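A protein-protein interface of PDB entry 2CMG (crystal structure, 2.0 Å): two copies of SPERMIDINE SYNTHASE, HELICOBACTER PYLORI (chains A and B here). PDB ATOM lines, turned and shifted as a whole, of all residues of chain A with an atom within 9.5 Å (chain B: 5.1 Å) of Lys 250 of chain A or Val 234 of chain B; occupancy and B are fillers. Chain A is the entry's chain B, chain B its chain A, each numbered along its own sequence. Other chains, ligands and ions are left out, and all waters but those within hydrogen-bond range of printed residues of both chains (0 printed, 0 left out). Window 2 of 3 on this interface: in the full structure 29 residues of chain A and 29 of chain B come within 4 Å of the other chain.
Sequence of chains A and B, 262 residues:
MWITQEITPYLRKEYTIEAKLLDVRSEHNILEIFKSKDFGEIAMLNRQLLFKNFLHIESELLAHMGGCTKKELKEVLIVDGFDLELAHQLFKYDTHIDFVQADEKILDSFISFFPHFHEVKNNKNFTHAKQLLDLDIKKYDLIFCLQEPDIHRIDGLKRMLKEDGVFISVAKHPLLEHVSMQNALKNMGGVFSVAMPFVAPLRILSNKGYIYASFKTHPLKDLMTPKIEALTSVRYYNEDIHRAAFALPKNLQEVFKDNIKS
Lys 250 of chain A touches just these residues of chain B: Val 234 (3.2 Å), Arg 235 (3.2 Å), Tyr 236 (3.1 Å) and Asn 238 (3.1 Å). Of chain A, only Lys 250 (3.2 Å) comes within 4 Å of Val 234 of chain B. Ser 233 of chain B touches none of the printed residues of chain A. Of the printed residues of chain B, Pro 249 of chain A touches Tyr 236 and Asn 238. Printed residues of chain A within 4 Å of Arg 235 of chain B: Lys 250 (3.2 Å) and Asn 251 (2.7 Å). Of the printed residues of chain A, Tyr 236 of chain B touches Pro 249 (3.4 Å) and Lys 250 (3.1 Å). Printed residues of chain A within 4 Å of Asn 238 of chain B: Leu 248, Pro 249 and Lys 250. Ala 247 of chain A touches none of the printed residues of chain B. Glu 60 of chain B touches none of the printed residues of chain A. The nearest residue of chain B that does not touch Lys 250 of chain A is Tyr 237 of chain B (4.4 Å).
Printed residues of chain B that touch a printed residue of chain A: Val 234, Arg 235, Tyr 236 and Asn 238. Hydrophobic or aromatic side chains of chain B within 4 Å of the printed part of chain A: Val 234 and Tyr 236. Hydrophobic or aromatic side chains of chain A within 4 Å of the printed part of chain B: Pro 249. Among the printed residues, 8 pairs touch across the chains. Among the printed residues, no Asp or Glu carboxylate lies within 4 Å of a Lys or Arg side-chain nitrogen of the other chain.
Among the printed residues, merely in contact across the chains: Pro 249 of chain A with Tyr 236 of chain B, Pro 249 of chain A with Asn 238 of chain B and Lys 250 of chain A with Arg 235 of chain B.
NZ of Lys 250 of chain A sits at hydrogen-bond distance from O of Val 234 of chain B (3.2 Å). The backbone carbonyl oxygen (O) of Arg 235 of chain B is in hydrogen-bond range of the backbone NH (N) of Asn 251 of chain A, at 2.7 Å. The backbone carbonyl oxygen (O) of Tyr 236 of chain B is in hydrogen-bond range of the backbone NH (N) of Lys 250 of chain A, 3.1 Å away. ND2 of Asn 238 of chain B is in hydrogen-bond range of O of Leu 248 of chain A (3.2 Å). The side-chain amide nitrogen (ND2) of Asn 238 of chain B lies close to the backbone NH (N) of Lys 250 of chain A (3.1 Å).
N of Arg 235 of chain B lies within hydrogen-bond range of OE2 of Glu 60 of chain B, at 2.7 Å. OE1 of Glu 60 of chain B lies within hydrogen-bond range of N of Tyr 236 of chain B (2.6 Å). ND2 of Asn 238 of chain B is in hydrogen-bond range of O of Tyr 236 of chain B (3.4 Å). NE2 of Gln 253 of chain A is in hydrogen-bond range of O of Leu 248 of chain A (2.9 Å).
No position is printed for both chains. Of the 8 pairs that touch across the chains among the printed residues, none has its exchanged pair printed and touching as well.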
ATOM      1  N   LEU A 175     -14.733 -27.785   5.823  1.00  0.00           N
ATOM      2  CA  LEU A 175     -15.004 -26.988   4.626  1.00  0.00           C
ATOM      3  C   LEU A 175     -13.710 -26.373   4.097  1.00  0.00           C
ATOM      4  O   LEU A 175     -13.397 -26.452   2.908  1.00  0.00           O
ATOM      5  CB  LEU A 175     -16.000 -25.866   4.933  1.00  0.00           C
ATOM      6  CG  LEU A 175     -16.494 -25.065   3.724  1.00  0.00           C
ATOM      7  CD1 LEU A 175     -17.491 -25.899   2.923  1.00  0.00           C
ATOM      8  CD2 LEU A 175     -17.134 -23.780   4.194  1.00  0.00           C
ATOM      9  N   ALA A 247     -24.144 -30.863  11.330  1.00  0.00           N
ATOM     10  CA  ALA A 247     -24.716 -30.431  10.057  1.00  0.00           C
ATOM     11  C   ALA A 247     -23.643 -30.262   8.979  1.00  0.00           C
ATOM     12  O   ALA A 247     -22.655 -29.552   9.167  1.00  0.00           O
ATOM     13  CB  ALA A 247     -25.485 -29.132  10.240  1.00  0.00           C
ATOM     14  N   LEU A 248     -23.844 -30.922   7.847  1.00  0.00           N
ATOM     15  CA  LEU A 248     -22.897 -30.857   6.739  1.00  0.00           C
ATOM     16  C   LEU A 248     -23.570 -30.435   5.437  1.00  0.00           C
ATOM     17  O   LEU A 248     -24.634 -30.950   5.087  1.00  0.00           O
ATOM     18  CB  LEU A 248     -22.242 -32.218   6.524  1.00  0.00           C
ATOM     19  CG  LEU A 248     -21.156 -32.819   7.413  1.00  0.00           C
ATOM     20  CD1 LEU A 248     -20.743 -34.175   6.802  1.00  0.00           C
ATOM     21  CD2 LEU A 248     -19.949 -31.905   7.474  1.00  0.00           C
ATOM     22  N   PRO A 249     -22.954 -29.490   4.701  1.00  0.00           N
ATOM     23  CA  PRO A 249     -23.512 -29.017   3.432  1.00  0.00           C
ATOM     24  C   PRO A 249     -23.541 -30.141   2.389  1.00  0.00           C
ATOM     25  O   PRO A 249     -22.789 -31.118   2.495  1.00  0.00           O
ATOM     26  CB  PRO A 249     -22.581 -27.867   3.057  1.00  0.00           C
ATOM     27  CG  PRO A 249     -21.293 -28.250   3.709  1.00  0.00           C
ATOM     28  CD  PRO A 249     -21.735 -28.740   5.048  1.00  0.00           C
ATOM     29  N   LYS A 250     -24.416 -29.993   1.396  1.00  0.00           N
ATOM     30  CA  LYS A 250     -24.590 -30.992   0.335  1.00  0.00           C
ATOM     31  C   LYS A 250     -23.285 -31.534  -0.244  1.00  0.00           C
ATOM     32  O   LYS A 250     -23.077 -32.749  -0.308  1.00  0.00           O
ATOM     33  CB  LYS A 250     -25.440 -30.397  -0.794  1.00  0.00           C
ATOM     34  CG  LYS A 250     -25.868 -31.400  -1.868  1.00  0.00           C
ATOM     35  CD  LYS A 250     -27.163 -30.957  -2.530  1.00  0.00           C
ATOM     36  CE  LYS A 250     -27.646 -31.947  -3.571  1.00  0.00           C
ATOM     37  NZ  LYS A 250     -26.858 -31.861  -4.826  1.00  0.00           N
ATOM     38  N   ASN A 251     -22.415 -30.617  -0.656  1.00  0.00           N
ATOM     39  CA  ASN A 251     -21.128 -30.965  -1.252  1.00  0.00           C
ATOM     40  C   ASN A 251     -20.240 -31.820  -0.353  1.00  0.00           C
ATOM     41  O   ASN A 251     -19.709 -32.835  -0.788  1.00  0.00           O
ATOM     42  CB  ASN A 251     -20.357 -29.701  -1.622  1.00  0.00           C
ATOM     43  CG  ASN A 251     -19.882 -28.947  -0.402  1.00  0.00           C
ATOM     44  OD1 ASN A 251     -20.673 -28.336   0.313  1.00  0.00           O
ATOM     45  ND2 ASN A 251     -18.588 -29.008  -0.144  1.00  0.00           N
ATOM     46  N   LEU A 252     -20.078 -31.399   0.897  1.00  0.00           N
ATOM     47  CA  LEU A 252     -19.231 -32.124   1.820  1.00  0.00           C
ATOM     48  C   LEU A 252     -19.792 -33.486   2.196  1.00  0.00           C
ATOM     49  O   LEU A 252     -19.034 -34.421   2.439  1.00  0.00           O
ATOM     50  CB  LEU A 252     -18.956 -31.276   3.066  1.00  0.00           C
ATOM     51  CG  LEU A 252     -18.012 -30.097   2.783  1.00  0.00           C
ATOM     52  CD1 LEU A 252     -17.731 -29.308   4.056  1.00  0.00           C
ATOM     53  CD2 LEU A 252     -16.708 -30.632   2.171  1.00  0.00           C
ATOM     54  N   GLN A 253     -21.114 -33.614   2.243  1.00  0.00           N
ATOM     55  CA  GLN A 253     -21.712 -34.906   2.568  1.00  0.00           C
ATOM     56  C   GLN A 253     -21.327 -35.876   1.457  1.00  0.00           C
ATOM     57  O   GLN A 253     -20.985 -37.033   1.701  1.00  0.00           O
ATOM     58  CB  GLN A 253     -23.230 -34.783   2.633  1.00  0.00           C
ATOM     59  CG  GLN A 253     -23.711 -33.838   3.706  1.00  0.00           C
ATOM     60  CD  GLN A 253     -24.883 -34.402   4.486  1.00  0.00           C
ATOM     61  OE1 GLN A 253     -24.866 -35.577   4.875  1.00  0.00           O
ATOM     62  NE2 GLN A 253     -25.904 -33.574   4.730  1.00  0.00           N
ATOM     63  N   GLU A 254     -21.388 -35.369   0.231  1.00  0.00           N
ATOM     64  CA  GLU A 254     -21.062 -36.120  -0.964  1.00  0.00           C
ATOM     65  C   GLU A 254     -19.607 -36.579  -0.997  1.00  0.00           C
ATOM     66  O   GLU A 254     -19.323 -37.763  -1.187  1.00  0.00           O
ATOM     67  CB  GLU A 254     -21.359 -35.249  -2.181  1.00  0.00           C
ATOM     68  CG  GLU A 254     -20.875 -35.814  -3.480  1.00  0.00           C
ATOM     69  CD  GLU A 254     -21.941 -35.767  -4.549  1.00  0.00           C
ATOM     70  OE1 GLU A 254     -22.421 -34.658  -4.887  1.00  0.00           O
ATOM     71  OE2 GLU A 254     -22.294 -36.856  -5.053  1.00  0.00           O
ATOM     72  N   VAL A 255     -18.690 -35.634  -0.818  1.00  0.00           N
ATOM     73  CA  VAL A 255     -17.258 -35.921  -0.831  1.00  0.00           C
ATOM     74  C   VAL A 255     -16.834 -36.839   0.306  1.00  0.00           C
ATOM     75  O   VAL A 255     -15.879 -37.607   0.171  1.00  0.00           O
ATOM     76  CB  VAL A 255     -16.425 -34.616  -0.718  1.00  0.00           C
ATOM     77  CG1 VAL A 255     -16.660 -33.953   0.628  1.00  0.00           C
ATOM     78  CG2 VAL A 255     -14.952 -34.927  -0.895  1.00  0.00           C
ATOM     79  N   PHE A 256     -17.553 -36.755   1.420  1.00  0.00           N
ATOM     80  CA  PHE A 256     -17.251 -37.561   2.596  1.00  0.00           C
ATOM     81  C   PHE A 256     -18.093 -38.848   2.679  1.00  0.00           C
ATOM     82  O   PHE A 256     -17.814 -39.709   3.509  1.00  0.00           O
ATOM     83  CB  PHE A 256     -17.497 -36.736   3.872  1.00  0.00           C
ATOM     84  CG  PHE A 256     -16.580 -35.537   4.039  1.00  0.00           C
ATOM     85  CD1 PHE A 256     -15.255 -35.572   3.604  1.00  0.00           C
ATOM     86  CD2 PHE A 256     -17.027 -34.403   4.716  1.00  0.00           C
ATOM     87  CE1 PHE A 256     -14.399 -34.498   3.853  1.00  0.00           C
ATOM     88  CE2 PHE A 256     -16.176 -33.328   4.967  1.00  0.00           C
ATOM     89  CZ  PHE A 256     -14.864 -33.374   4.539  1.00  0.00           C
ATOM     90  N   LYS A 257     -19.099 -38.977   1.813  1.00  0.00           N
ATOM     91  CA  LYS A 257     -20.029 -40.111   1.816  1.00  0.00           C
ATOM     92  C   LYS A 257     -19.502 -41.524   1.992  1.00  0.00           C
ATOM     93  O   LYS A 257     -20.240 -42.398   2.449  1.00  0.00           O
ATOM     94  CB  LYS A 257     -20.921 -40.080   0.565  1.00  0.00           C
ATOM     95  CG  LYS A 257     -20.242 -40.481  -0.739  1.00  0.00           C
ATOM     96  CD  LYS A 257     -21.247 -40.411  -1.873  1.00  0.00           C
ATOM     97  CE  LYS A 257     -20.678 -40.902  -3.195  1.00  0.00           C
ATOM     98  NZ  LYS A 257     -19.610 -40.002  -3.723  1.00  0.00           N
ATOM     99  N   ILE A 260     -17.906 -41.567   5.959  1.00  0.00           N
ATOM    100  CA  ILE A 260     -18.761 -41.402   7.124  1.00  0.00           C
ATOM    101  C   ILE A 260     -19.546 -42.652   7.492  1.00  0.00           C
ATOM    102  O   ILE A 260     -20.329 -43.186   6.701  1.00  0.00           O
ATOM    103  CB  ILE A 260     -19.748 -40.220   6.942  1.00  0.00           C
ATOM    104  CG1 ILE A 260     -18.978 -38.901   6.890  1.00  0.00           C
ATOM    105  CG2 ILE A 260     -20.731 -40.172   8.106  1.00  0.00           C
ATOM    106  CD1 ILE A 260     -19.765 -37.716   6.331  1.00  0.00           C
ATOM    107  N   GLU B  60     -26.964 -19.476  -1.753  1.00  0.00           N
ATOM    108  CA  GLU B  60     -27.866 -20.596  -1.572  1.00  0.00           C
ATOM    109  C   GLU B  60     -28.609 -20.438  -0.237  1.00  0.00           C
ATOM    110  O   GLU B  60     -29.833 -20.548  -0.188  1.00  0.00           O
ATOM    111  CB  GLU B  60     -27.110 -21.936  -1.614  1.00  0.00           C
ATOM    112  CG  GLU B  60     -26.791 -22.468  -3.041  1.00  0.00           C
ATOM    113  CD  GLU B  60     -26.071 -23.812  -3.012  1.00  0.00           C
ATOM    114  OE1 GLU B  60     -26.296 -24.551  -2.032  1.00  0.00           O
ATOM    115  OE2 GLU B  60     -25.299 -24.141  -3.961  1.00  0.00           O
ATOM    116  N   HIS B  64     -32.715 -19.749  -0.483  1.00  0.00           N
ATOM    117  CA  HIS B  64     -33.610 -20.844  -0.174  1.00  0.00           C
ATOM    118  C   HIS B  64     -34.121 -20.826   1.260  1.00  0.00           C
ATOM    119  O   HIS B  64     -34.950 -21.641   1.638  1.00  0.00           O
ATOM    120  CB  HIS B  64     -32.917 -22.152  -0.517  1.00  0.00           C
ATOM    121  CG  HIS B  64     -32.436 -22.203  -1.934  1.00  0.00           C
ATOM    122  ND1 HIS B  64     -31.149 -22.556  -2.273  1.00  0.00           N
ATOM    123  CD2 HIS B  64     -33.048 -21.865  -3.095  1.00  0.00           C
ATOM    124  CE1 HIS B  64     -30.985 -22.427  -3.578  1.00  0.00           C
ATOM    125  NE2 HIS B  64     -32.123 -22.009  -4.100  1.00  0.00           N
ATOM    126  N   GLN B  89     -30.068 -17.996  -7.615  1.00  0.00           N
ATOM    127  CA  GLN B  89     -30.647 -19.072  -6.832  1.00  0.00           C
ATOM    128  C   GLN B  89     -32.163 -18.903  -6.692  1.00  0.00           C
ATOM    129  O   GLN B  89     -32.905 -19.884  -6.603  1.00  0.00           O
ATOM    130  CB  GLN B  89     -29.994 -19.109  -5.448  1.00  0.00           C
ATOM    131  CG  GLN B  89     -28.504 -19.422  -5.462  1.00  0.00           C
ATOM    132  CD  GLN B  89     -28.196 -20.824  -5.963  1.00  0.00           C
ATOM    133  OE1 GLN B  89     -28.980 -21.746  -5.765  1.00  0.00           O
ATOM    134  NE2 GLN B  89     -27.042 -20.990  -6.597  1.00  0.00           N
ATOM    135  N   LYS B  92     -34.680 -20.167  -9.320  1.00  0.00           N
ATOM    136  CA  LYS B  92     -34.916 -21.596  -9.340  1.00  0.00           C
ATOM    137  C   LYS B  92     -36.347 -21.790  -8.848  1.00  0.00           C
ATOM    138  O   LYS B  92     -36.801 -22.906  -8.654  1.00  0.00           O
ATOM    139  CB  LYS B  92     -33.930 -22.331  -8.437  1.00  0.00           C
ATOM    140  CG  LYS B  92     -32.506 -22.371  -8.980  1.00  0.00           C
ATOM    141  CD  LYS B  92     -31.611 -23.168  -8.058  1.00  0.00           C
ATOM    142  CE  LYS B  92     -30.185 -23.210  -8.575  1.00  0.00           C
ATOM    143  NZ  LYS B  92     -29.325 -23.904  -7.591  1.00  0.00           N
ATOM    144  N   LEU B 231     -34.668 -28.970  -5.281  1.00  0.00           N
ATOM    145  CA  LEU B 231     -33.528 -28.257  -5.837  1.00  0.00           C
ATOM    146  C   LEU B 231     -32.412 -29.260  -6.105  1.00  0.00           C
ATOM    147  O   LEU B 231     -31.813 -29.808  -5.172  1.00  0.00           O
ATOM    148  CB  LEU B 231     -33.039 -27.193  -4.852  1.00  0.00           C
ATOM    149  CG  LEU B 231     -34.070 -26.259  -4.220  1.00  0.00           C
ATOM    150  CD1 LEU B 231     -33.402 -25.515  -3.077  1.00  0.00           C
ATOM    151  CD2 LEU B 231     -34.647 -25.281  -5.249  1.00  0.00           C
ATOM    152  N   THR B 232     -32.121 -29.487  -7.381  1.00  0.00           N
ATOM    153  CA  THR B 232     -31.086 -30.440  -7.768  1.00  0.00           C
ATOM    154  C   THR B 232     -29.850 -29.780  -8.372  1.00  0.00           C
ATOM    155  O   THR B 232     -29.037 -30.442  -9.033  1.00  0.00           O
ATOM    156  CB  THR B 232     -31.645 -31.454  -8.768  1.00  0.00           C
ATOM    157  OG1 THR B 232     -32.551 -30.789  -9.655  1.00  0.00           O
ATOM    158  CG2 THR B 232     -32.363 -32.581  -8.038  1.00  0.00           C
ATOM    159  N   SER B 233     -29.701 -28.483  -8.117  1.00  0.00           N
ATOM    160  CA  SER B 233     -28.590 -27.713  -8.652  1.00  0.00           C
ATOM    161  C   SER B 233     -27.830 -26.973  -7.555  1.00  0.00           C
ATOM    162  O   SER B 233     -26.960 -26.141  -7.846  1.00  0.00           O
ATOM    163  CB  SER B 233     -29.135 -26.720  -9.663  1.00  0.00           C
ATOM    164  OG  SER B 233     -30.277 -26.076  -9.120  1.00  0.00           O
ATOM    165  N   VAL B 234     -28.166 -27.281  -6.302  1.00  0.00           N
ATOM    166  CA  VAL B 234     -27.532 -26.658  -5.140  1.00  0.00           C
ATOM    167  C   VAL B 234     -26.366 -27.494  -4.626  1.00  0.00           C
ATOM    168  O   VAL B 234     -26.386 -28.726  -4.695  1.00  0.00           O
ATOM    169  CB  VAL B 234     -28.540 -26.452  -3.969  1.00  0.00           C
ATOM    170  CG1 VAL B 234     -29.668 -25.506  -4.395  1.00  0.00           C
ATOM    171  CG2 VAL B 234     -29.108 -27.791  -3.534  1.00  0.00           C
ATOM    172  N   ARG B 235     -25.365 -26.811  -4.078  1.00  0.00           N
ATOM    173  CA  ARG B 235     -24.162 -27.466  -3.572  1.00  0.00           C
ATOM    174  C   ARG B 235     -23.954 -27.404  -2.057  1.00  0.00           C
ATOM    175  O   ARG B 235     -23.232 -28.230  -1.488  1.00  0.00           O
ATOM    176  CB  ARG B 235     -22.929 -26.877  -4.259  1.00  0.00           C
ATOM    177  CG  ARG B 235     -22.778 -27.286  -5.715  1.00  0.00           C
ATOM    178  CD  ARG B 235     -21.608 -26.564  -6.366  1.00  0.00           C
ATOM    179  NE  ARG B 235     -21.914 -25.152  -6.545  1.00  0.00           N
ATOM    180  CZ  ARG B 235     -21.019 -24.225  -6.859  1.00  0.00           C
ATOM    181  NH1 ARG B 235     -19.744 -24.557  -7.027  1.00  0.00           N
ATOM    182  NH2 ARG B 235     -21.405 -22.962  -7.013  1.00  0.00           N
ATOM    183  N   TYR B 236     -24.593 -26.435  -1.414  1.00  0.00           N
ATOM    184  CA  TYR B 236     -24.457 -26.235   0.018  1.00  0.00           C
ATOM    185  C   TYR B 236     -25.764 -26.421   0.778  1.00  0.00           C
ATOM    186  O   TYR B 236     -25.853 -27.255   1.659  1.00  0.00           O
ATOM    187  CB  TYR B 236     -23.872 -24.830   0.240  1.00  0.00           C
ATOM    188  CG  TYR B 236     -23.868 -24.303   1.655  1.00  0.00           C
ATOM    189  CD1 TYR B 236     -24.959 -23.585   2.151  1.00  0.00           C
ATOM    190  CD2 TYR B 236     -22.775 -24.499   2.493  1.00  0.00           C
ATOM    191  CE1 TYR B 236     -24.964 -23.074   3.447  1.00  0.00           C
ATOM    192  CE2 TYR B 236     -22.765 -23.992   3.799  1.00  0.00           C
ATOM    193  CZ  TYR B 236     -23.869 -23.278   4.269  1.00  0.00           C
ATOM    194  OH  TYR B 236     -23.886 -22.757   5.548  1.00  0.00           O
ATOM    195  N   TYR B 237     -26.785 -25.660   0.409  1.00  0.00           N
ATOM    196  CA  TYR B 237     -28.082 -25.712   1.077  1.00  0.00           C
ATOM    197  C   TYR B 237     -28.823 -27.051   1.118  1.00  0.00           C
ATOM    198  O   TYR B 237     -28.885 -27.774   0.129  1.00  0.00           O
ATOM    199  CB  TYR B 237     -29.021 -24.670   0.459  1.00  0.00           C
ATOM    200  CG  TYR B 237     -30.365 -24.590   1.146  1.00  0.00           C
ATOM    201  CD1 TYR B 237     -30.497 -23.967   2.387  1.00  0.00           C
ATOM    202  CD2 TYR B 237     -31.499 -25.163   0.574  1.00  0.00           C
ATOM    203  CE1 TYR B 237     -31.723 -23.923   3.043  1.00  0.00           C
ATOM    204  CE2 TYR B 237     -32.735 -25.121   1.223  1.00  0.00           C
ATOM    205  CZ  TYR B 237     -32.833 -24.501   2.456  1.00  0.00           C
ATOM    206  OH  TYR B 237     -34.042 -24.465   3.115  1.00  0.00           O
ATOM    207  N   ASN B 238     -29.389 -27.348   2.290  1.00  0.00           N
ATOM    208  CA  ASN B 238     -30.199 -28.542   2.558  1.00  0.00           C
ATOM    209  C   ASN B 238     -30.917 -28.303   3.885  1.00  0.00           C
ATOM    210  O   ASN B 238     -30.739 -27.252   4.492  1.00  0.00           O
ATOM    211  CB  ASN B 238     -29.363 -29.838   2.604  1.00  0.00           C
ATOM    212  CG  ASN B 238     -28.210 -29.788   3.593  1.00  0.00           C
ATOM    213  OD1 ASN B 238     -28.390 -29.518   4.783  1.00  0.00           O
ATOM    214  ND2 ASN B 238     -27.008 -30.082   3.099  1.00  0.00           N
